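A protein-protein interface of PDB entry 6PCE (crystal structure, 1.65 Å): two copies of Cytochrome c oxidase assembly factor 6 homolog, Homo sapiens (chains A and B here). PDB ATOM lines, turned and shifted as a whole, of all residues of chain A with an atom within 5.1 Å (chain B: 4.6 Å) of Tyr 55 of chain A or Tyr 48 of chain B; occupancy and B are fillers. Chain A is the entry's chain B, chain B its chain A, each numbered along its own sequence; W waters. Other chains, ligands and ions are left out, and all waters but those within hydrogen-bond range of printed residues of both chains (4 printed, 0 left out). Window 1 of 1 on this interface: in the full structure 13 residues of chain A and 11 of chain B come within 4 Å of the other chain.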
ATOM      1  N   LYS A  51      27.209  19.586 -29.695  1.00  0.00           N
ATOM      2  CA  LYS A  51      27.555  21.029 -29.918  1.00  0.00           C
ATOM      3  C   LYS A  51      26.421  21.711 -30.682  1.00  0.00           C
ATOM      4  O   LYS A  51      26.088  22.878 -30.367  1.00  0.00           O
ATOM      5  CB  LYS A  51      28.881  21.162 -30.643  1.00  0.00           C
ATOM      6  CG  LYS A  51      30.043  20.751 -29.752  1.00  0.00           C
ATOM      7  CD  LYS A  51      31.325  20.782 -30.460  1.00  0.00           C
ATOM      8  CE  LYS A  51      32.467  20.232 -29.621  1.00  0.00           C
ATOM      9  NZ  LYS A  51      32.851  21.161 -28.533  1.00  0.00           N
ATOM     10  N   ARG A  52      25.865  21.024 -31.686  1.00  0.00           N
ATOM     11  CA  ARG A  52      24.761  21.619 -32.491  1.00  0.00           C
ATOM     12  C   ARG A  52      23.579  21.832 -31.539  1.00  0.00           C
ATOM     13  O   ARG A  52      22.925  22.909 -31.602  1.00  0.00           O
ATOM     14  CB  ARG A  52      24.400  20.748 -33.692  1.00  0.00           C
ATOM     15  CG  ARG A  52      23.287  21.371 -34.533  1.00  0.00           C
ATOM     16  CD  ARG A  52      23.065  20.936 -35.963  1.00  0.00           C
ATOM     17  NE  ARG A  52      22.064  21.846 -36.544  1.00  0.00           N
ATOM     18  CZ  ARG A  52      22.320  23.008 -37.161  1.00  0.00           C
ATOM     19  NH1 ARG A  52      23.555  23.417 -37.380  1.00  0.00           N
ATOM     20  NH2 ARG A  52      21.314  23.749 -37.608  1.00  0.00           N
ATOM     21  N   ARG A  53      23.268  20.881 -30.675  1.00  0.00           N
ATOM     22  CA  ARG A  53      22.120  20.969 -29.718  1.00  0.00           C
ATOM     23  C   ARG A  53      22.288  22.225 -28.853  1.00  0.00           C
ATOM     24  O   ARG A  53      21.328  22.989 -28.678  1.00  0.00           O
ATOM     25  CB  ARG A  53      22.035  19.723 -28.821  1.00  0.00           C
ATOM     26  CG  ARG A  53      20.911  19.707 -27.788  1.00  0.00           C
ATOM     27  CD  ARG A  53      19.531  19.763 -28.424  1.00  0.00           C
ATOM     28  NE  ARG A  53      18.401  19.628 -27.495  1.00  0.00           N
ATOM     29  CZ  ARG A  53      17.153  19.356 -27.875  1.00  0.00           C
ATOM     30  NH1 ARG A  53      16.862  19.181 -29.148  1.00  0.00           N
ATOM     31  NH2 ARG A  53      16.188  19.238 -26.981  1.00  0.00           N
ATOM     32  N   ASP A  54      23.485  22.406 -28.301  1.00  0.00           N
ATOM     33  CA  ASP A  54      23.754  23.550 -27.394  1.00  0.00           C
ATOM     34  C   ASP A  54      23.529  24.840 -28.159  1.00  0.00           C
ATOM     35  O   ASP A  54      22.910  25.779 -27.611  1.00  0.00           O
ATOM     36  CB  ASP A  54      25.170  23.532 -26.833  1.00  0.00           C
ATOM     37  CG  ASP A  54      25.311  22.705 -25.578  1.00  0.00           C
ATOM     38  OD1 ASP A  54      24.287  22.169 -25.122  1.00  0.00           O
ATOM     39  OD2 ASP A  54      26.451  22.604 -25.078  1.00  0.00           O
ATOM     40  N   TYR A  55      24.048  24.917 -29.365  1.00  0.00           N
ATOM     41  CA  TYR A  55      23.892  26.108 -30.235  1.00  0.00           C
ATOM     42  C   TYR A  55      22.405  26.367 -30.435  1.00  0.00           C
ATOM     43  O   TYR A  55      21.917  27.502 -30.136  1.00  0.00           O
ATOM     44  CB  TYR A  55      24.617  25.914 -31.556  1.00  0.00           C
ATOM     45  CG  TYR A  55      24.065  26.744 -32.671  1.00  0.00           C
ATOM     46  CD1 TYR A  55      24.052  28.118 -32.542  1.00  0.00           C
ATOM     47  CD2 TYR A  55      23.601  26.167 -33.838  1.00  0.00           C
ATOM     48  CE1 TYR A  55      23.524  28.910 -33.540  1.00  0.00           C
ATOM     49  CE2 TYR A  55      23.085  26.953 -34.856  1.00  0.00           C
ATOM     50  CZ  TYR A  55      23.067  28.328 -34.705  1.00  0.00           C
ATOM     51  OH  TYR A  55      22.599  29.156 -35.690  1.00  0.00           O
ATOM     52  N   LEU A  56      21.662  25.338 -30.834  1.00  0.00           N
ATOM     53  CA  LEU A  56      20.228  25.543 -31.207  1.00  0.00           C
ATOM     54  C   LEU A  56      19.427  25.950 -29.978  1.00  0.00           C
ATOM     55  O   LEU A  56      18.563  26.837 -30.115  1.00  0.00           O
ATOM     56  CB  LEU A  56      19.623  24.282 -31.829  1.00  0.00           C
ATOM     57  CG  LEU A  56      20.131  23.933 -33.220  1.00  0.00           C
ATOM     58  CD1 LEU A  56      19.480  22.644 -33.701  1.00  0.00           C
ATOM     59  CD2 LEU A  56      19.891  25.069 -34.213  1.00  0.00           C
ATOM     60  N   LYS A  57      19.704  25.377 -28.805  1.00  0.00           N
ATOM     61  CA  LYS A  57      18.968  25.689 -27.558  1.00  0.00           C
ATOM     62  C   LYS A  57      19.218  27.140 -27.150  1.00  0.00           C
ATOM     63  O   LYS A  57      18.264  27.842 -26.707  1.00  0.00           O
ATOM     64  CB  LYS A  57      19.400  24.790 -26.399  1.00  0.00           C
ATOM     65  CG  LYS A  57      18.797  23.390 -26.409  1.00  0.00           C
ATOM     66  CD  LYS A  57      17.295  23.348 -26.654  1.00  0.00           C
ATOM     67  CE  LYS A  57      16.509  24.218 -25.696  1.00  0.00           C
ATOM     68  NZ  LYS A  57      15.063  23.913 -25.717  1.00  0.00           N
ATOM     69  N   PHE A  58      20.467  27.584 -27.247  1.00  0.00           N
ATOM     70  CA  PHE A  58      20.821  28.942 -26.796  1.00  0.00           C
ATOM     71  C   PHE A  58      20.327  29.923 -27.838  1.00  0.00           C
ATOM     72  O   PHE A  58      20.030  31.047 -27.488  1.00  0.00           O
ATOM     73  CB  PHE A  58      22.297  29.074 -26.432  1.00  0.00           C
ATOM     74  CG  PHE A  58      22.607  28.542 -25.059  1.00  0.00           C
ATOM     75  CD1 PHE A  58      22.919  27.200 -24.877  1.00  0.00           C
ATOM     76  CD2 PHE A  58      22.525  29.362 -23.945  1.00  0.00           C
ATOM     77  CE1 PHE A  58      23.181  26.707 -23.605  1.00  0.00           C
ATOM     78  CE2 PHE A  58      22.791  28.868 -22.676  1.00  0.00           C
ATOM     79  CZ  PHE A  58      23.122  27.541 -22.510  1.00  0.00           C
ATOM     80  N   LYS A  59      20.284  29.512 -29.096  1.00  0.00           N
ATOM     81  CA  LYS A  59      19.714  30.378 -30.145  1.00  0.00           C
ATOM     82  C   LYS A  59      18.230  30.563 -29.833  1.00  0.00           C
ATOM     83  O   LYS A  59      17.735  31.703 -29.896  1.00  0.00           O
ATOM     84  CB  LYS A  59      19.894  29.742 -31.507  1.00  0.00           C
ATOM     85  CG  LYS A  59      19.305  30.595 -32.622  1.00  0.00           C
ATOM     86  CD  LYS A  59      19.783  30.181 -33.978  1.00  0.00           C
ATOM     87  CE  LYS A  59      19.063  28.970 -34.519  1.00  0.00           C
ATOM     88  NZ  LYS A  59      17.922  29.377 -35.369  1.00  0.00           N
ATOM     89  N   GLU A  60      17.531  29.469 -29.565  1.00  0.00           N
ATOM     90  CA  GLU A  60      16.080  29.532 -29.223  1.00  0.00           C
ATOM     91  C   GLU A  60      15.852  30.448 -28.022  1.00  0.00           C
ATOM     92  O   GLU A  60      14.846  31.219 -28.060  1.00  0.00           O
ATOM     93  CB  GLU A  60      15.523  28.129 -29.008  1.00  0.00           C
ATOM     94  CG  GLU A  60      15.203  27.444 -30.331  1.00  0.00           C
ATOM     95  CD  GLU A  60      15.184  25.926 -30.325  1.00  0.00           C
ATOM     96  OE1 GLU A  60      14.892  25.341 -29.271  1.00  0.00           O
ATOM     97  OE2 GLU A  60      15.448  25.339 -31.391  1.00  0.00           O
ATOM     98  N   PHE A  62      17.755  32.947 -27.007  1.00  0.00           N
ATOM     99  CA  PHE A  62      18.090  34.298 -27.529  1.00  0.00           C
ATOM    100  C   PHE A  62      16.899  34.863 -28.312  1.00  0.00           C
ATOM    101  O   PHE A  62      16.457  36.008 -28.032  1.00  0.00           O
ATOM    102  CB  PHE A  62      19.347  34.187 -28.396  1.00  0.00           C
ATOM    103  CG  PHE A  62      19.666  35.344 -29.309  1.00  0.00           C
ATOM    104  CD1 PHE A  62      20.013  36.586 -28.803  1.00  0.00           C
ATOM    105  CD2 PHE A  62      19.686  35.155 -30.686  1.00  0.00           C
ATOM    106  CE1 PHE A  62      20.341  37.624 -29.666  1.00  0.00           C
ATOM    107  CE2 PHE A  62      20.030  36.192 -31.540  1.00  0.00           C
ATOM    108  CZ  PHE A  62      20.377  37.417 -31.024  1.00  0.00           C
ATOM    109  N   GLN B  44      22.658  36.689 -22.106  1.00  0.00           N
ATOM    110  CA  GLN B  44      21.922  35.683 -22.909  1.00  0.00           C
ATOM    111  C   GLN B  44      22.552  35.629 -24.310  1.00  0.00           C
ATOM    112  O   GLN B  44      22.757  34.522 -24.835  1.00  0.00           O
ATOM    113  CB  GLN B  44      20.443  36.067 -22.966  1.00  0.00           C
ATOM    114  CG  GLN B  44      19.508  34.928 -23.329  1.00  0.00           C
ATOM    115  CD  GLN B  44      18.080  35.417 -23.325  1.00  0.00           C
ATOM    116  OE1 GLN B  44      17.699  36.282 -24.112  1.00  0.00           O
ATOM    117  NE2 GLN B  44      17.281  34.881 -22.416  1.00  0.00           N
ATOM    118  N   TRP B  45      22.877  36.790 -24.881  1.00  0.00           N
ATOM    119  CA  TRP B  45      23.510  36.880 -26.215  1.00  0.00           C
ATOM    120  C   TRP B  45      24.934  36.290 -26.161  1.00  0.00           C
ATOM    121  O   TRP B  45      25.304  35.603 -27.105  1.00  0.00           O
ATOM    122  CB  TRP B  45      23.521  38.314 -26.729  1.00  0.00           C
ATOM    123  CG  TRP B  45      22.170  38.936 -26.907  1.00  0.00           C
ATOM    124  CD1 TRP B  45      20.999  38.691 -26.239  1.00  0.00           C
ATOM    125  CD2 TRP B  45      21.905  40.018 -27.804  1.00  0.00           C
ATOM    126  NE1 TRP B  45      20.008  39.516 -26.710  1.00  0.00           N
ATOM    127  CE2 TRP B  45      20.540  40.361 -27.655  1.00  0.00           C
ATOM    128  CE3 TRP B  45      22.679  40.678 -28.759  1.00  0.00           C
ATOM    129  CZ2 TRP B  45      19.949  41.363 -28.419  1.00  0.00           C
ATOM    130  CZ3 TRP B  45      22.096  41.682 -29.496  1.00  0.00           C
ATOM    131  CH2 TRP B  45      20.749  42.007 -29.334  1.00  0.00           C
ATOM    132  N   ILE B  46      25.741  36.634 -25.159  1.00  0.00           N
ATOM    133  CA  ILE B  46      27.134  36.129 -25.049  1.00  0.00           C
ATOM    134  C   ILE B  46      27.077  34.605 -25.045  1.00  0.00           C
ATOM    135  O   ILE B  46      27.915  34.003 -25.695  1.00  0.00           O
ATOM    136  CB  ILE B  46      27.848  36.622 -23.779  1.00  0.00           C
ATOM    137  CG1 ILE B  46      28.024  38.145 -23.771  1.00  0.00           C
ATOM    138  CG2 ILE B  46      29.168  35.891 -23.595  1.00  0.00           C
ATOM    139  CD1 ILE B  46      29.010  38.643 -24.799  1.00  0.00           C
ATOM    140  N   LYS B  47      26.144  34.005 -24.292  1.00  0.00           N
ATOM    141  CA  LYS B  47      26.059  32.517 -24.206  1.00  0.00           C
ATOM    142  C   LYS B  47      25.720  31.973 -25.593  1.00  0.00           C
ATOM    143  O   LYS B  47      26.353  31.003 -26.015  1.00  0.00           O
ATOM    144  CB  LYS B  47      25.033  32.057 -23.155  1.00  0.00           C
ATOM    145  N   TYR B  48      24.779  32.585 -26.309  1.00  0.00           N
ATOM    146  CA  TYR B  48      24.383  32.167 -27.678  1.00  0.00           C
ATOM    147  C   TYR B  48      25.611  32.239 -28.603  1.00  0.00           C
ATOM    148  O   TYR B  48      25.938  31.279 -29.309  1.00  0.00           O
ATOM    149  CB  TYR B  48      23.214  33.013 -28.154  1.00  0.00           C
ATOM    150  CG  TYR B  48      23.022  33.106 -29.643  1.00  0.00           C
ATOM    151  CD1 TYR B  48      22.764  31.994 -30.444  1.00  0.00           C
ATOM    152  CD2 TYR B  48      23.131  34.329 -30.264  1.00  0.00           C
ATOM    153  CE1 TYR B  48      22.621  32.119 -31.819  1.00  0.00           C
ATOM    154  CE2 TYR B  48      22.965  34.473 -31.627  1.00  0.00           C
ATOM    155  CZ  TYR B  48      22.701  33.368 -32.409  1.00  0.00           C
ATOM    156  OH  TYR B  48      22.538  33.567 -33.751  1.00  0.00           O
ATOM    157  N   PHE B  49      26.292  33.376 -28.598  1.00  0.00           N
ATOM    158  CA  PHE B  49      27.451  33.571 -29.505  1.00  0.00           C
ATOM    159  C   PHE B  49      28.559  32.561 -29.161  1.00  0.00           C
ATOM    160  O   PHE B  49      29.179  31.967 -30.075  1.00  0.00           O
ATOM    161  CB  PHE B  49      28.004  34.982 -29.350  1.00  0.00           C
ATOM    162  CG  PHE B  49      27.099  36.074 -29.840  1.00  0.00           C
ATOM    163  CD1 PHE B  49      26.416  35.936 -31.034  1.00  0.00           C
ATOM    164  CD2 PHE B  49      26.969  37.257 -29.125  1.00  0.00           C
ATOM    165  CE1 PHE B  49      25.635  36.976 -31.518  1.00  0.00           C
ATOM    166  CE2 PHE B  49      26.203  38.305 -29.613  1.00  0.00           C
ATOM    167  CZ  PHE B  49      25.528  38.153 -30.810  1.00  0.00           C
ATOM    168  N   ASP B  50      28.850  32.388 -27.880  1.00  0.00           N
ATOM    169  CA  ASP B  50      29.884  31.413 -27.455  1.00  0.00           C
ATOM    170  C   ASP B  50      29.541  29.995 -27.936  1.00  0.00           C
ATOM    171  O   ASP B  50      30.456  29.270 -28.388  1.00  0.00           O
ATOM    172  CB  ASP B  50      30.114  31.431 -25.962  1.00  0.00           C
ATOM    173  CG  ASP B  50      30.870  32.644 -25.439  1.00  0.00           C
ATOM    174  OD1 ASP B  50      31.436  33.428 -26.276  1.00  0.00           O
ATOM    175  OD2 ASP B  50      30.931  32.778 -24.179  1.00  0.00           O
ATOM    176  N   LYS B  51      28.283  29.576 -27.817  1.00  0.00           N
ATOM    177  CA  LYS B  51      27.864  28.235 -28.297  1.00  0.00           C
ATOM    178  C   LYS B  51      27.919  28.152 -29.818  1.00  0.00           C
ATOM    179  O   LYS B  51      28.259  27.102 -30.329  1.00  0.00           O
ATOM    180  CB  LYS B  51      26.482  27.905 -27.762  1.00  0.00           C
ATOM    181  CG  LYS B  51      26.437  27.640 -26.259  1.00  0.00           C
ATOM    182  CD  LYS B  51      27.326  26.513 -25.801  1.00  0.00           C
ATOM    183  CE  LYS B  51      27.196  26.253 -24.315  1.00  0.00           C
ATOM    184  NZ  LYS B  51      27.930  25.025 -23.947  1.00  0.00           N
ATOM    185  N   ARG B  52      27.579  29.238 -30.522  1.00  0.00           N
ATOM    186  CA  ARG B  52      27.727  29.272 -31.992  1.00  0.00           C
ATOM    187  C   ARG B  52      29.201  29.085 -32.357  1.00  0.00           C
ATOM    188  O   ARG B  52      29.509  28.283 -33.224  1.00  0.00           O
ATOM    189  CB  ARG B  52      27.172  30.579 -32.542  1.00  0.00           C
ATOM    190  CG  ARG B  52      27.409  30.723 -34.043  1.00  0.00           C
ATOM    191  CD  ARG B  52      26.585  29.804 -34.903  1.00  0.00           C
ATOM    192  NE  ARG B  52      27.046  29.694 -36.290  1.00  0.00           N
ATOM    193  CZ  ARG B  52      26.608  28.783 -37.167  1.00  0.00           C
ATOM    194  NH1 ARG B  52      25.679  27.918 -36.804  1.00  0.00           N
ATOM    195  NH2 ARG B  52      27.104  28.732 -38.397  1.00  0.00           N
ATOM    196  N   TYR B  55      30.404  25.508 -31.822  1.00  0.00           N
ATOM    197  CA  TYR B  55      29.815  24.654 -32.878  1.00  0.00           C
ATOM    198  C   TYR B  55      30.573  24.868 -34.192  1.00  0.00           C
ATOM    199  O   TYR B  55      30.963  23.914 -34.838  1.00  0.00           O
ATOM    200  CB  TYR B  55      28.333  24.934 -33.038  1.00  0.00           C
ATOM    201  CG  TYR B  55      27.723  24.252 -34.228  1.00  0.00           C
ATOM    202  CD1 TYR B  55      27.601  22.875 -34.255  1.00  0.00           C
ATOM    203  CD2 TYR B  55      27.307  24.971 -35.333  1.00  0.00           C
ATOM    204  CE1 TYR B  55      27.058  22.224 -35.352  1.00  0.00           C
ATOM    205  CE2 TYR B  55      26.749  24.334 -36.434  1.00  0.00           C
ATOM    206  CZ  TYR B  55      26.623  22.960 -36.442  1.00  0.00           C
ATOM    207  OH  TYR B  55      26.076  22.323 -37.529  1.00  0.00           O
HETATM  208  O   HOH W   1      27.904  24.675 -29.153  1.00  0.00           O
HETATM  209  O   HOH W   2      23.435  31.699 -35.412  1.00  0.00           O
HETATM  210  O   HOH W   3      20.989  32.391 -24.947  1.00  0.00           O
HETATM  211  O   HOH W   4      17.289  37.728 -26.233  1.00  0.00           O
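OD2 of Asp 54 of chain A is in salt-bridge range of NZ of Lys 51 of chain B (3.1 Å).
OH of Tyr 55 of chain B sits at hydrogen-bond distance from NH1 of Arg 52 of chain A (2.8 Å).
Water W4 lies within hydrogen-bond range of the side-chain amide oxygen (OE1) of Gln 44 of chain B (2.6 Å), the backbone carbonyl oxygen (O) of Phe 62 of chain A (2.6 Å) and the indole nitrogen (NE1) of Trp 45 of chain B (3.3 Å).
Water W2 lies within hydrogen-bond range of OH of Tyr 48 of chain B and OH of Tyr 55 of chain A.
Water W1 bridges the backbone carbonyl oxygen (O) of Lys 51 of chain B (2.7 Å) and the backbone carbonyl oxygen (O) of Lys 51 of chain A (2.8 Å).
Water W3 bridges the backbone carbonyl oxygen (O) of Gln 44 of chain B (2.8 Å) and the backbone carbonyl oxygen (O) of Phe 58 of chain A (3.0 Å).
Of the 10 printed residues of chain B, 7 touch a printed residue of chain A.
Hydrophobic or aromatic side chains of chain B that line the printed part of chain A: Trp 45, Tyr 48 and Tyr 55.
Of the 11 printed residues of chain A, 7 touch a printed residue of chain B.
Hydrophobic or aromatic side chains of chain A that line the printed part of chain B: Tyr 55, Phe 58 and Phe 62.
Among the printed residues, Asp or Glu carboxylates within 4 Å of a Lys or Arg side-chain nitrogen of the other chain: Asp 54 of chain A with Lys 51 of chain B (3.1 Å).
Printed residues of chain B within 4 Å of Lys 51 of chain A: Tyr 55 (3.9 Å).
Of the printed residues of chain B, Tyr 55 of chain A touches Tyr 48 (3.8 Å) and Arg 52 (3.4 Å).
Of the printed residues of chain B, Lys 59 of chain A touches Tyr 48 (3.5 Å).
Ile 46 of chain B touches none of the printed residues of chain A.
Tyr 48 of chain B touches just these residues of chain A: Tyr 55, Phe 58, Lys 59 and Phe 62.
The nearest printed residue of chain B that does not touch Lys 59 of chain A is Lys 51 of chain B (6.5 Å).
C of Lys 51 of chain A touches CD1 of Tyr 55 of chain B (3.9 Å).
Tyr 48 of chain B touches Tyr 55 of chain A.
Tyr 55 of chain A touches Arg 52 of chain B (CZ to NH1, 3.4 Å).
CD2 of Phe 58 of chain A touches CB of Lys 47 of chain B (3.8 Å).
Phe 58 of chain A touches Tyr 48 of chain B (O to CB, 3.8 Å).
Phe 58 of chain A touches Lys 51 of chain B (CD1 to CG, 3.8 Å).
Tyr 48 of chain B touches Lys 59 of chain A.
Gln 44 of chain B touches Phe 62 of chain A.
Trp 45 of chain B touches Phe 62 of chain A.
CE2 of Phe 62 of chain A touches CE2 of Tyr 48 of chain B, 3.4 Å away.
Lys 51 of chain A touches Tyr 55 of chain B, but with the chains exchanged Tyr 55 of chain A does not touch Lys 51 of chain B (4.01 Å).
Arg 52 of chain A touches Tyr 55 of chain B, and with the chains exchanged Tyr 55 of chain A touches Arg 52 of chain B.
Positions printed for both chains: 51, 52 and 55.
Of the 12 pairs that touch across the chains among the printed residues, 2 have their exchanged pair printed and touching as well.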
